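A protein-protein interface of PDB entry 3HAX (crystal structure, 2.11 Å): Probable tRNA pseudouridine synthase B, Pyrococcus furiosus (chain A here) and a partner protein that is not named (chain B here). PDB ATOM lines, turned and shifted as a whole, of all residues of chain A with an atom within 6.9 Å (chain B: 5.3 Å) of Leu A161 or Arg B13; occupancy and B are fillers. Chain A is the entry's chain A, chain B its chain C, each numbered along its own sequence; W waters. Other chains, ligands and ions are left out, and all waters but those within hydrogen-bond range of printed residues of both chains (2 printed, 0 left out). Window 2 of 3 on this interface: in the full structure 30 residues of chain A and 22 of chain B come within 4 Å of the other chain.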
ATOM      1  N   VAL A 111       8.535  19.772   8.881  1.00  0.00           N
ATOM      2  CA  VAL A 111       7.366  20.023   9.709  1.00  0.00           C
ATOM      3  C   VAL A 111       6.230  20.340   8.745  1.00  0.00           C
ATOM      4  O   VAL A 111       6.363  21.215   7.887  1.00  0.00           O
ATOM      5  CB  VAL A 111       7.599  21.166  10.731  1.00  0.00           C
ATOM      6  CG1 VAL A 111       6.298  21.560  11.422  1.00  0.00           C
ATOM      7  CG2 VAL A 111       8.622  20.737  11.776  1.00  0.00           C
ATOM      8  N   ALA A 112       5.129  19.604   8.870  1.00  0.00           N
ATOM      9  CA  ALA A 112       4.023  19.703   7.925  1.00  0.00           C
ATOM     10  C   ALA A 112       2.692  19.966   8.608  1.00  0.00           C
ATOM     11  O   ALA A 112       2.466  19.545   9.744  1.00  0.00           O
ATOM     12  CB  ALA A 112       3.934  18.438   7.085  1.00  0.00           C
ATOM     13  N   GLU A 159       6.279  12.261  14.093  1.00  0.00           N
ATOM     14  CA  GLU A 159       5.852  12.740  15.401  1.00  0.00           C
ATOM     15  C   GLU A 159       4.742  13.771  15.242  1.00  0.00           C
ATOM     16  O   GLU A 159       4.961  14.844  14.680  1.00  0.00           O
ATOM     17  CB  GLU A 159       7.030  13.342  16.174  1.00  0.00           C
ATOM     18  CG  GLU A 159       6.679  13.784  17.596  1.00  0.00           C
ATOM     19  CD  GLU A 159       7.775  14.599  18.269  1.00  0.00           C
ATOM     20  OE1 GLU A 159       7.846  14.569  19.516  1.00  0.00           O
ATOM     21  OE2 GLU A 159       8.560  15.267  17.565  1.00  0.00           O
ATOM     22  N   VAL A 160       3.552  13.434  15.732  1.00  0.00           N
ATOM     23  CA  VAL A 160       2.438  14.378  15.760  1.00  0.00           C
ATOM     24  C   VAL A 160       2.681  15.384  16.885  1.00  0.00           C
ATOM     25  O   VAL A 160       2.853  15.006  18.048  1.00  0.00           O
ATOM     26  CB  VAL A 160       1.074  13.666  15.944  1.00  0.00           C
ATOM     27  CG1 VAL A 160      -0.059  14.682  16.052  1.00  0.00           C
ATOM     28  CG2 VAL A 160       0.813  12.701  14.791  1.00  0.00           C
ATOM     29  N   LEU A 161       2.715  16.663  16.523  1.00  0.00           N
ATOM     30  CA  LEU A 161       2.976  17.726  17.484  1.00  0.00           C
ATOM     31  C   LEU A 161       1.684  18.185  18.149  1.00  0.00           C
ATOM     32  O   LEU A 161       1.574  18.164  19.377  1.00  0.00           O
ATOM     33  CB  LEU A 161       3.720  18.893  16.820  1.00  0.00           C
ATOM     34  CG  LEU A 161       5.125  18.567  16.293  1.00  0.00           C
ATOM     35  CD1 LEU A 161       5.667  19.687  15.412  1.00  0.00           C
ATOM     36  CD2 LEU A 161       6.094  18.256  17.436  1.00  0.00           C
ATOM     37  N   GLU A 162       0.707  18.585  17.338  1.00  0.00           N
ATOM     38  CA  GLU A 162      -0.619  18.940  17.843  1.00  0.00           C
ATOM     39  C   GLU A 162      -1.721  18.780  16.801  1.00  0.00           C
ATOM     40  O   GLU A 162      -1.466  18.799  15.594  1.00  0.00           O
ATOM     41  CB  GLU A 162      -0.641  20.350  18.460  1.00  0.00           C
ATOM     42  CG  GLU A 162      -0.070  21.462  17.596  1.00  0.00           C
ATOM     43  CD  GLU A 162       0.041  22.778  18.353  1.00  0.00           C
ATOM     44  OE1 GLU A 162      -0.668  23.736  17.982  1.00  0.00           O
ATOM     45  OE2 GLU A 162       0.823  22.853  19.327  1.00  0.00           O
ATOM     46  N   ILE A 163      -2.945  18.604  17.291  1.00  0.00           N
ATOM     47  CA  ILE A 163      -4.119  18.461  16.444  1.00  0.00           C
ATOM     48  C   ILE A 163      -5.163  19.495  16.853  1.00  0.00           C
ATOM     49  O   ILE A 163      -5.545  19.573  18.022  1.00  0.00           O
ATOM     50  CB  ILE A 163      -4.715  17.022  16.519  1.00  0.00           C
ATOM     51  CG1 ILE A 163      -3.675  15.982  16.077  1.00  0.00           C
ATOM     52  CG2 ILE A 163      -5.993  16.909  15.672  1.00  0.00           C
ATOM     53  CD1 ILE A 163      -4.006  14.548  16.459  1.00  0.00           C
ATOM     54  N   VAL A 168      -3.695  18.804  11.413  1.00  0.00           N
ATOM     55  CA  VAL A 168      -2.699  18.000  12.110  1.00  0.00           C
ATOM     56  C   VAL A 168      -1.297  18.515  11.799  1.00  0.00           C
ATOM     57  O   VAL A 168      -0.856  18.487  10.646  1.00  0.00           O
ATOM     58  CB  VAL A 168      -2.807  16.500  11.725  1.00  0.00           C
ATOM     59  CG1 VAL A 168      -1.738  15.670  12.440  1.00  0.00           C
ATOM     60  CG2 VAL A 168      -4.201  15.960  12.029  1.00  0.00           C
ATOM     61  N   LEU A 169      -0.610  18.990  12.836  1.00  0.00           N
ATOM     62  CA  LEU A 169       0.771  19.437  12.714  1.00  0.00           C
ATOM     63  C   LEU A 169       1.712  18.310  13.128  1.00  0.00           C
ATOM     64  O   LEU A 169       1.602  17.773  14.236  1.00  0.00           O
ATOM     65  CB  LEU A 169       1.014  20.685  13.574  1.00  0.00           C
ATOM     66  CG  LEU A 169       2.395  21.349  13.502  1.00  0.00           C
ATOM     67  CD1 LEU A 169       2.617  22.047  12.165  1.00  0.00           C
ATOM     68  CD2 LEU A 169       2.559  22.328  14.650  1.00  0.00           C
ATOM     69  N   PHE A 170       2.626  17.944  12.237  1.00  0.00           N
ATOM     70  CA  PHE A 170       3.542  16.844  12.525  1.00  0.00           C
ATOM     71  C   PHE A 170       4.945  17.042  11.960  1.00  0.00           C
ATOM     72  O   PHE A 170       5.140  17.742  10.966  1.00  0.00           O
ATOM     73  CB  PHE A 170       2.945  15.490  12.096  1.00  0.00           C
ATOM     74  CG  PHE A 170       2.846  15.296  10.604  1.00  0.00           C
ATOM     75  CD1 PHE A 170       3.814  14.560   9.923  1.00  0.00           C
ATOM     76  CD2 PHE A 170       1.774  15.818   9.887  1.00  0.00           C
ATOM     77  CE1 PHE A 170       3.728  14.362   8.549  1.00  0.00           C
ATOM     78  CE2 PHE A 170       1.676  15.625   8.510  1.00  0.00           C
ATOM     79  CZ  PHE A 170       2.657  14.896   7.841  1.00  0.00           C
ATOM     80  N   ARG A 171       5.913  16.429  12.634  1.00  0.00           N
ATOM     81  CA  ARG A 171       7.296  16.394  12.189  1.00  0.00           C
ATOM     82  C   ARG A 171       7.537  15.042  11.524  1.00  0.00           C
ATOM     83  O   ARG A 171       7.000  14.022  11.967  1.00  0.00           O
ATOM     84  CB  ARG A 171       8.232  16.582  13.389  1.00  0.00           C
ATOM     85  CG  ARG A 171       9.619  17.095  13.041  1.00  0.00           C
ATOM     86  CD  ARG A 171      10.492  17.240  14.285  1.00  0.00           C
ATOM     87  NE  ARG A 171      10.272  18.498  15.004  1.00  0.00           N
ATOM     88  CZ  ARG A 171      10.991  19.610  14.837  1.00  0.00           C
ATOM     89  NH1 ARG A 171      11.992  19.652  13.965  1.00  0.00           N
ATOM     90  NH2 ARG A 171      10.707  20.692  15.549  1.00  0.00           N
ATOM     91  N   ARG B   6       3.606  28.077  13.343  1.00  0.00           N
ATOM     92  CA  ARG B   6       4.310  29.031  14.191  1.00  0.00           C
ATOM     93  C   ARG B   6       5.461  28.343  14.919  1.00  0.00           C
ATOM     94  O   ARG B   6       5.444  27.127  15.120  1.00  0.00           O
ATOM     95  CB  ARG B   6       3.351  29.663  15.205  1.00  0.00           C
ATOM     96  CG  ARG B   6       2.281  30.541  14.579  1.00  0.00           C
ATOM     97  CD  ARG B   6       1.560  31.386  15.614  1.00  0.00           C
ATOM     98  NE  ARG B   6       1.046  32.615  15.012  1.00  0.00           N
ATOM     99  CZ  ARG B   6       1.556  33.827  15.214  1.00  0.00           C
ATOM    100  NH1 ARG B   6       2.591  34.000  16.026  1.00  0.00           N
ATOM    101  NH2 ARG B   6       1.015  34.877  14.611  1.00  0.00           N
ATOM    102  N   LYS B   7       6.458  29.132  15.306  1.00  0.00           N
ATOM    103  CA  LYS B   7       7.617  28.620  16.022  1.00  0.00           C
ATOM    104  C   LYS B   7       7.930  29.502  17.225  1.00  0.00           C
ATOM    105  O   LYS B   7       7.905  30.731  17.134  1.00  0.00           O
ATOM    106  CB  LYS B   7       8.834  28.531  15.094  1.00  0.00           C
ATOM    107  CG  LYS B   7       9.995  27.728  15.672  1.00  0.00           C
ATOM    108  CD  LYS B   7      11.248  27.851  14.825  1.00  0.00           C
ATOM    109  CE  LYS B   7      12.392  27.059  15.434  1.00  0.00           C
ATOM    110  NZ  LYS B   7      13.654  27.200  14.656  1.00  0.00           N
ATOM    111  N   CYS B   8       8.211  28.861  18.354  1.00  0.00           N
ATOM    112  CA  CYS B   8       8.615  29.567  19.559  1.00  0.00           C
ATOM    113  C   CYS B   8      10.052  30.077  19.430  1.00  0.00           C
ATOM    114  O   CYS B   8      10.948  29.311  19.077  1.00  0.00           O
ATOM    115  CB  CYS B   8       8.489  28.645  20.762  1.00  0.00           C
ATOM    116  SG  CYS B   8       9.043  29.346  22.318  1.00  0.00           S
ATOM    117  N   CYS B  11      12.315  28.149  22.816  1.00  0.00           N
ATOM    118  CA  CYS B  11      12.676  26.728  22.845  1.00  0.00           C
ATOM    119  C   CYS B  11      12.690  26.041  21.474  1.00  0.00           C
ATOM    120  O   CYS B  11      13.168  24.909  21.353  1.00  0.00           O
ATOM    121  CB  CYS B  11      11.767  25.961  23.808  1.00  0.00           C
ATOM    122  SG  CYS B  11      10.090  25.710  23.207  1.00  0.00           S
ATOM    123  N   GLY B  12      12.158  26.714  20.456  1.00  0.00           N
ATOM    124  CA  GLY B  12      12.150  26.185  19.092  1.00  0.00           C
ATOM    125  C   GLY B  12      11.014  25.226  18.769  1.00  0.00           C
ATOM    126  O   GLY B  12      11.043  24.549  17.741  1.00  0.00           O
ATOM    127  N   ARG B  13      10.012  25.174  19.644  1.00  0.00           N
ATOM    128  CA  ARG B  13       8.841  24.319  19.452  1.00  0.00           C
ATOM    129  C   ARG B  13       7.973  24.802  18.290  1.00  0.00           C
ATOM    130  O   ARG B  13       7.681  25.993  18.179  1.00  0.00           O
ATOM    131  CB  ARG B  13       8.009  24.266  20.742  1.00  0.00           C
ATOM    132  CG  ARG B  13       6.673  23.534  20.635  1.00  0.00           C
ATOM    133  CD  ARG B  13       6.843  22.028  20.735  1.00  0.00           C
ATOM    134  NE  ARG B  13       5.558  21.336  20.670  1.00  0.00           N
ATOM    135  CZ  ARG B  13       5.363  20.067  21.019  1.00  0.00           C
ATOM    136  NH1 ARG B  13       6.369  19.328  21.470  1.00  0.00           N
ATOM    137  NH2 ARG B  13       4.152  19.537  20.918  1.00  0.00           N
ATOM    138  N   TYR B  14       7.580  23.869  17.426  1.00  0.00           N
ATOM    139  CA  TYR B  14       6.604  24.144  16.379  1.00  0.00           C
ATOM    140  C   TYR B  14       5.196  23.903  16.900  1.00  0.00           C
ATOM    141  O   TYR B  14       4.911  22.864  17.508  1.00  0.00           O
ATOM    142  CB  TYR B  14       6.875  23.295  15.135  1.00  0.00           C
ATOM    143  CG  TYR B  14       7.946  23.875  14.243  1.00  0.00           C
ATOM    144  CD1 TYR B  14       9.268  23.447  14.339  1.00  0.00           C
ATOM    145  CD2 TYR B  14       7.639  24.864  13.315  1.00  0.00           C
ATOM    146  CE1 TYR B  14      10.256  23.985  13.523  1.00  0.00           C
ATOM    147  CE2 TYR B  14       8.615  25.409  12.494  1.00  0.00           C
ATOM    148  CZ  TYR B  14       9.919  24.967  12.604  1.00  0.00           C
ATOM    149  OH  TYR B  14      10.880  25.510  11.792  1.00  0.00           O
ATOM    150  N   THR B  15       4.322  24.874  16.651  1.00  0.00           N
ATOM    151  CA  THR B  15       2.972  24.887  17.204  1.00  0.00           C
ATOM    152  C   THR B  15       2.041  25.721  16.325  1.00  0.00           C
ATOM    153  O   THR B  15       2.501  26.482  15.474  1.00  0.00           O
ATOM    154  CB  THR B  15       2.966  25.435  18.658  1.00  0.00           C
ATOM    155  OG1 THR B  15       1.629  25.443  19.172  1.00  0.00           O
ATOM    156  CG2 THR B  15       3.540  26.849  18.720  1.00  0.00           C
ATOM    157  N   CYS B  20       3.449  29.421  23.316  1.00  0.00           N
ATOM    158  CA  CYS B  20       4.121  28.118  23.285  1.00  0.00           C
ATOM    159  C   CYS B  20       3.626  27.170  24.383  1.00  0.00           C
ATOM    160  O   CYS B  20       3.605  27.540  25.558  1.00  0.00           O
ATOM    161  CB  CYS B  20       5.633  28.312  23.389  1.00  0.00           C
ATOM    162  SG  CYS B  20       6.632  26.805  23.406  1.00  0.00           S
ATOM    163  N   PRO B  21       3.216  25.944  23.998  1.00  0.00           N
ATOM    164  CA  PRO B  21       2.724  24.962  24.968  1.00  0.00           C
ATOM    165  C   PRO B  21       3.822  24.350  25.846  1.00  0.00           C
ATOM    166  O   PRO B  21       3.512  23.668  26.824  1.00  0.00           O
ATOM    167  CB  PRO B  21       2.080  23.890  24.083  1.00  0.00           C
ATOM    168  CG  PRO B  21       2.791  23.985  22.792  1.00  0.00           C
ATOM    169  CD  PRO B  21       3.177  25.424  22.619  1.00  0.00           C
ATOM    170  N   VAL B  22       5.087  24.594  25.497  1.00  0.00           N
ATOM    171  CA  VAL B  22       6.220  24.070  26.266  1.00  0.00           C
ATOM    172  C   VAL B  22       6.722  25.081  27.302  1.00  0.00           C
ATOM    173  O   VAL B  22       6.784  24.767  28.490  1.00  0.00           O
ATOM    174  CB  VAL B  22       7.385  23.597  25.344  1.00  0.00           C
ATOM    175  CG1 VAL B  22       8.590  23.141  26.166  1.00  0.00           C
ATOM    176  CG2 VAL B  22       6.921  22.474  24.424  1.00  0.00           C
HETATM  177  O   HOH W   1       3.291  22.011  19.456  1.00  0.00           O
HETATM  178  O   HOH W   2       8.745  21.215  17.425  1.00  0.00           O
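CG2 of Val A111 touches CD1 of Tyr B14 (3.8 Å).
Leu A161 touches Tyr B14.
Leu A169 touches Tyr B14.
Thr B15 touches Leu A169.
Tyr B14 touches Arg A171.
O of Leu A161 sits at hydrogen-bond distance from NH2 of Arg B13 (3.3 Å).
OE2 of Glu A162 is in hydrogen-bond range of OG1 of Thr B15 (2.7 Å).
The backbone carbonyl oxygen of Glu A159 sits at hydrogen-bond distance from the backbone NH of Arg A171, at 2.8 Å.
N of Leu A161 is in hydrogen-bond range of O of Leu A169 (2.8 Å).
The backbone NH (N) of Leu A169 lies within hydrogen-bond range of the backbone carbonyl oxygen (O) of Glu A162, at 2.9 Å.
The backbone NH (N) of Arg B6 is in hydrogen-bond range of the backbone carbonyl oxygen (O) of Thr B15 (2.9 Å).
N of Cys B8 sits at hydrogen-bond distance from O of Arg B13 (2.9 Å).
The side-chain sulfur (SG) of Cys B11 lies close to the backbone NH (N) of Arg B13 (3.6 Å).
Arg B13 touches just one residue of chain A: Leu A161.
Gly B12 touches none of the printed residues of chain A.
Of the printed residues of chain A, Tyr B14 touches Val A111 (3.8 Å), Leu A161 (3.8 Å), Leu A169 (3.7 Å) and Arg A171 (3.3 Å).
Of the printed residues of chain B, Arg A171 touches Tyr B14.
Printed residues of chain B within 4 Å of Leu A169: Tyr B14 and Thr B15.
Val A168 touches none of the printed residues of chain B.
Phe A170 touches none of the printed residues of chain B.
The nearest residue of chain A that does not touch Arg B13 is Glu A162 (5.0 Å).
Of the 11 printed residues of chain B, 3 touch a printed residue of chain A.
Hydrophobic or aromatic side chains of chain B within 4 Å of the printed part of chain A: Tyr B14.
Of the 11 printed residues of chain A, 5 touch a printed residue of chain B.
Hydrophobic or aromatic side chains of chain A within 4 Å of the printed part of chain B: Val A111, Leu A161 and Leu A169.
Among the printed residues, 7 pairs touch across the chains.
Among the printed residues, no Asp or Glu carboxylate lies within 4 Å of a Lys or Arg side-chain nitrogen of the other chain.
Water W1 lies within hydrogen-bond range of the side-chain carboxylate (OE2) of Glu A162 (2.6 Å), the guanidinium group (NE) of Arg B13 (2.7 Å) and the backbone carbonyl oxygen (O) of Tyr B14 (2.7 Å).
Water W2 lies within hydrogen-bond range of the guanidinium group (NH2) of Arg A171 (2.8 Å) and the backbone NH (N) of Tyr B14 (2.9 Å).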
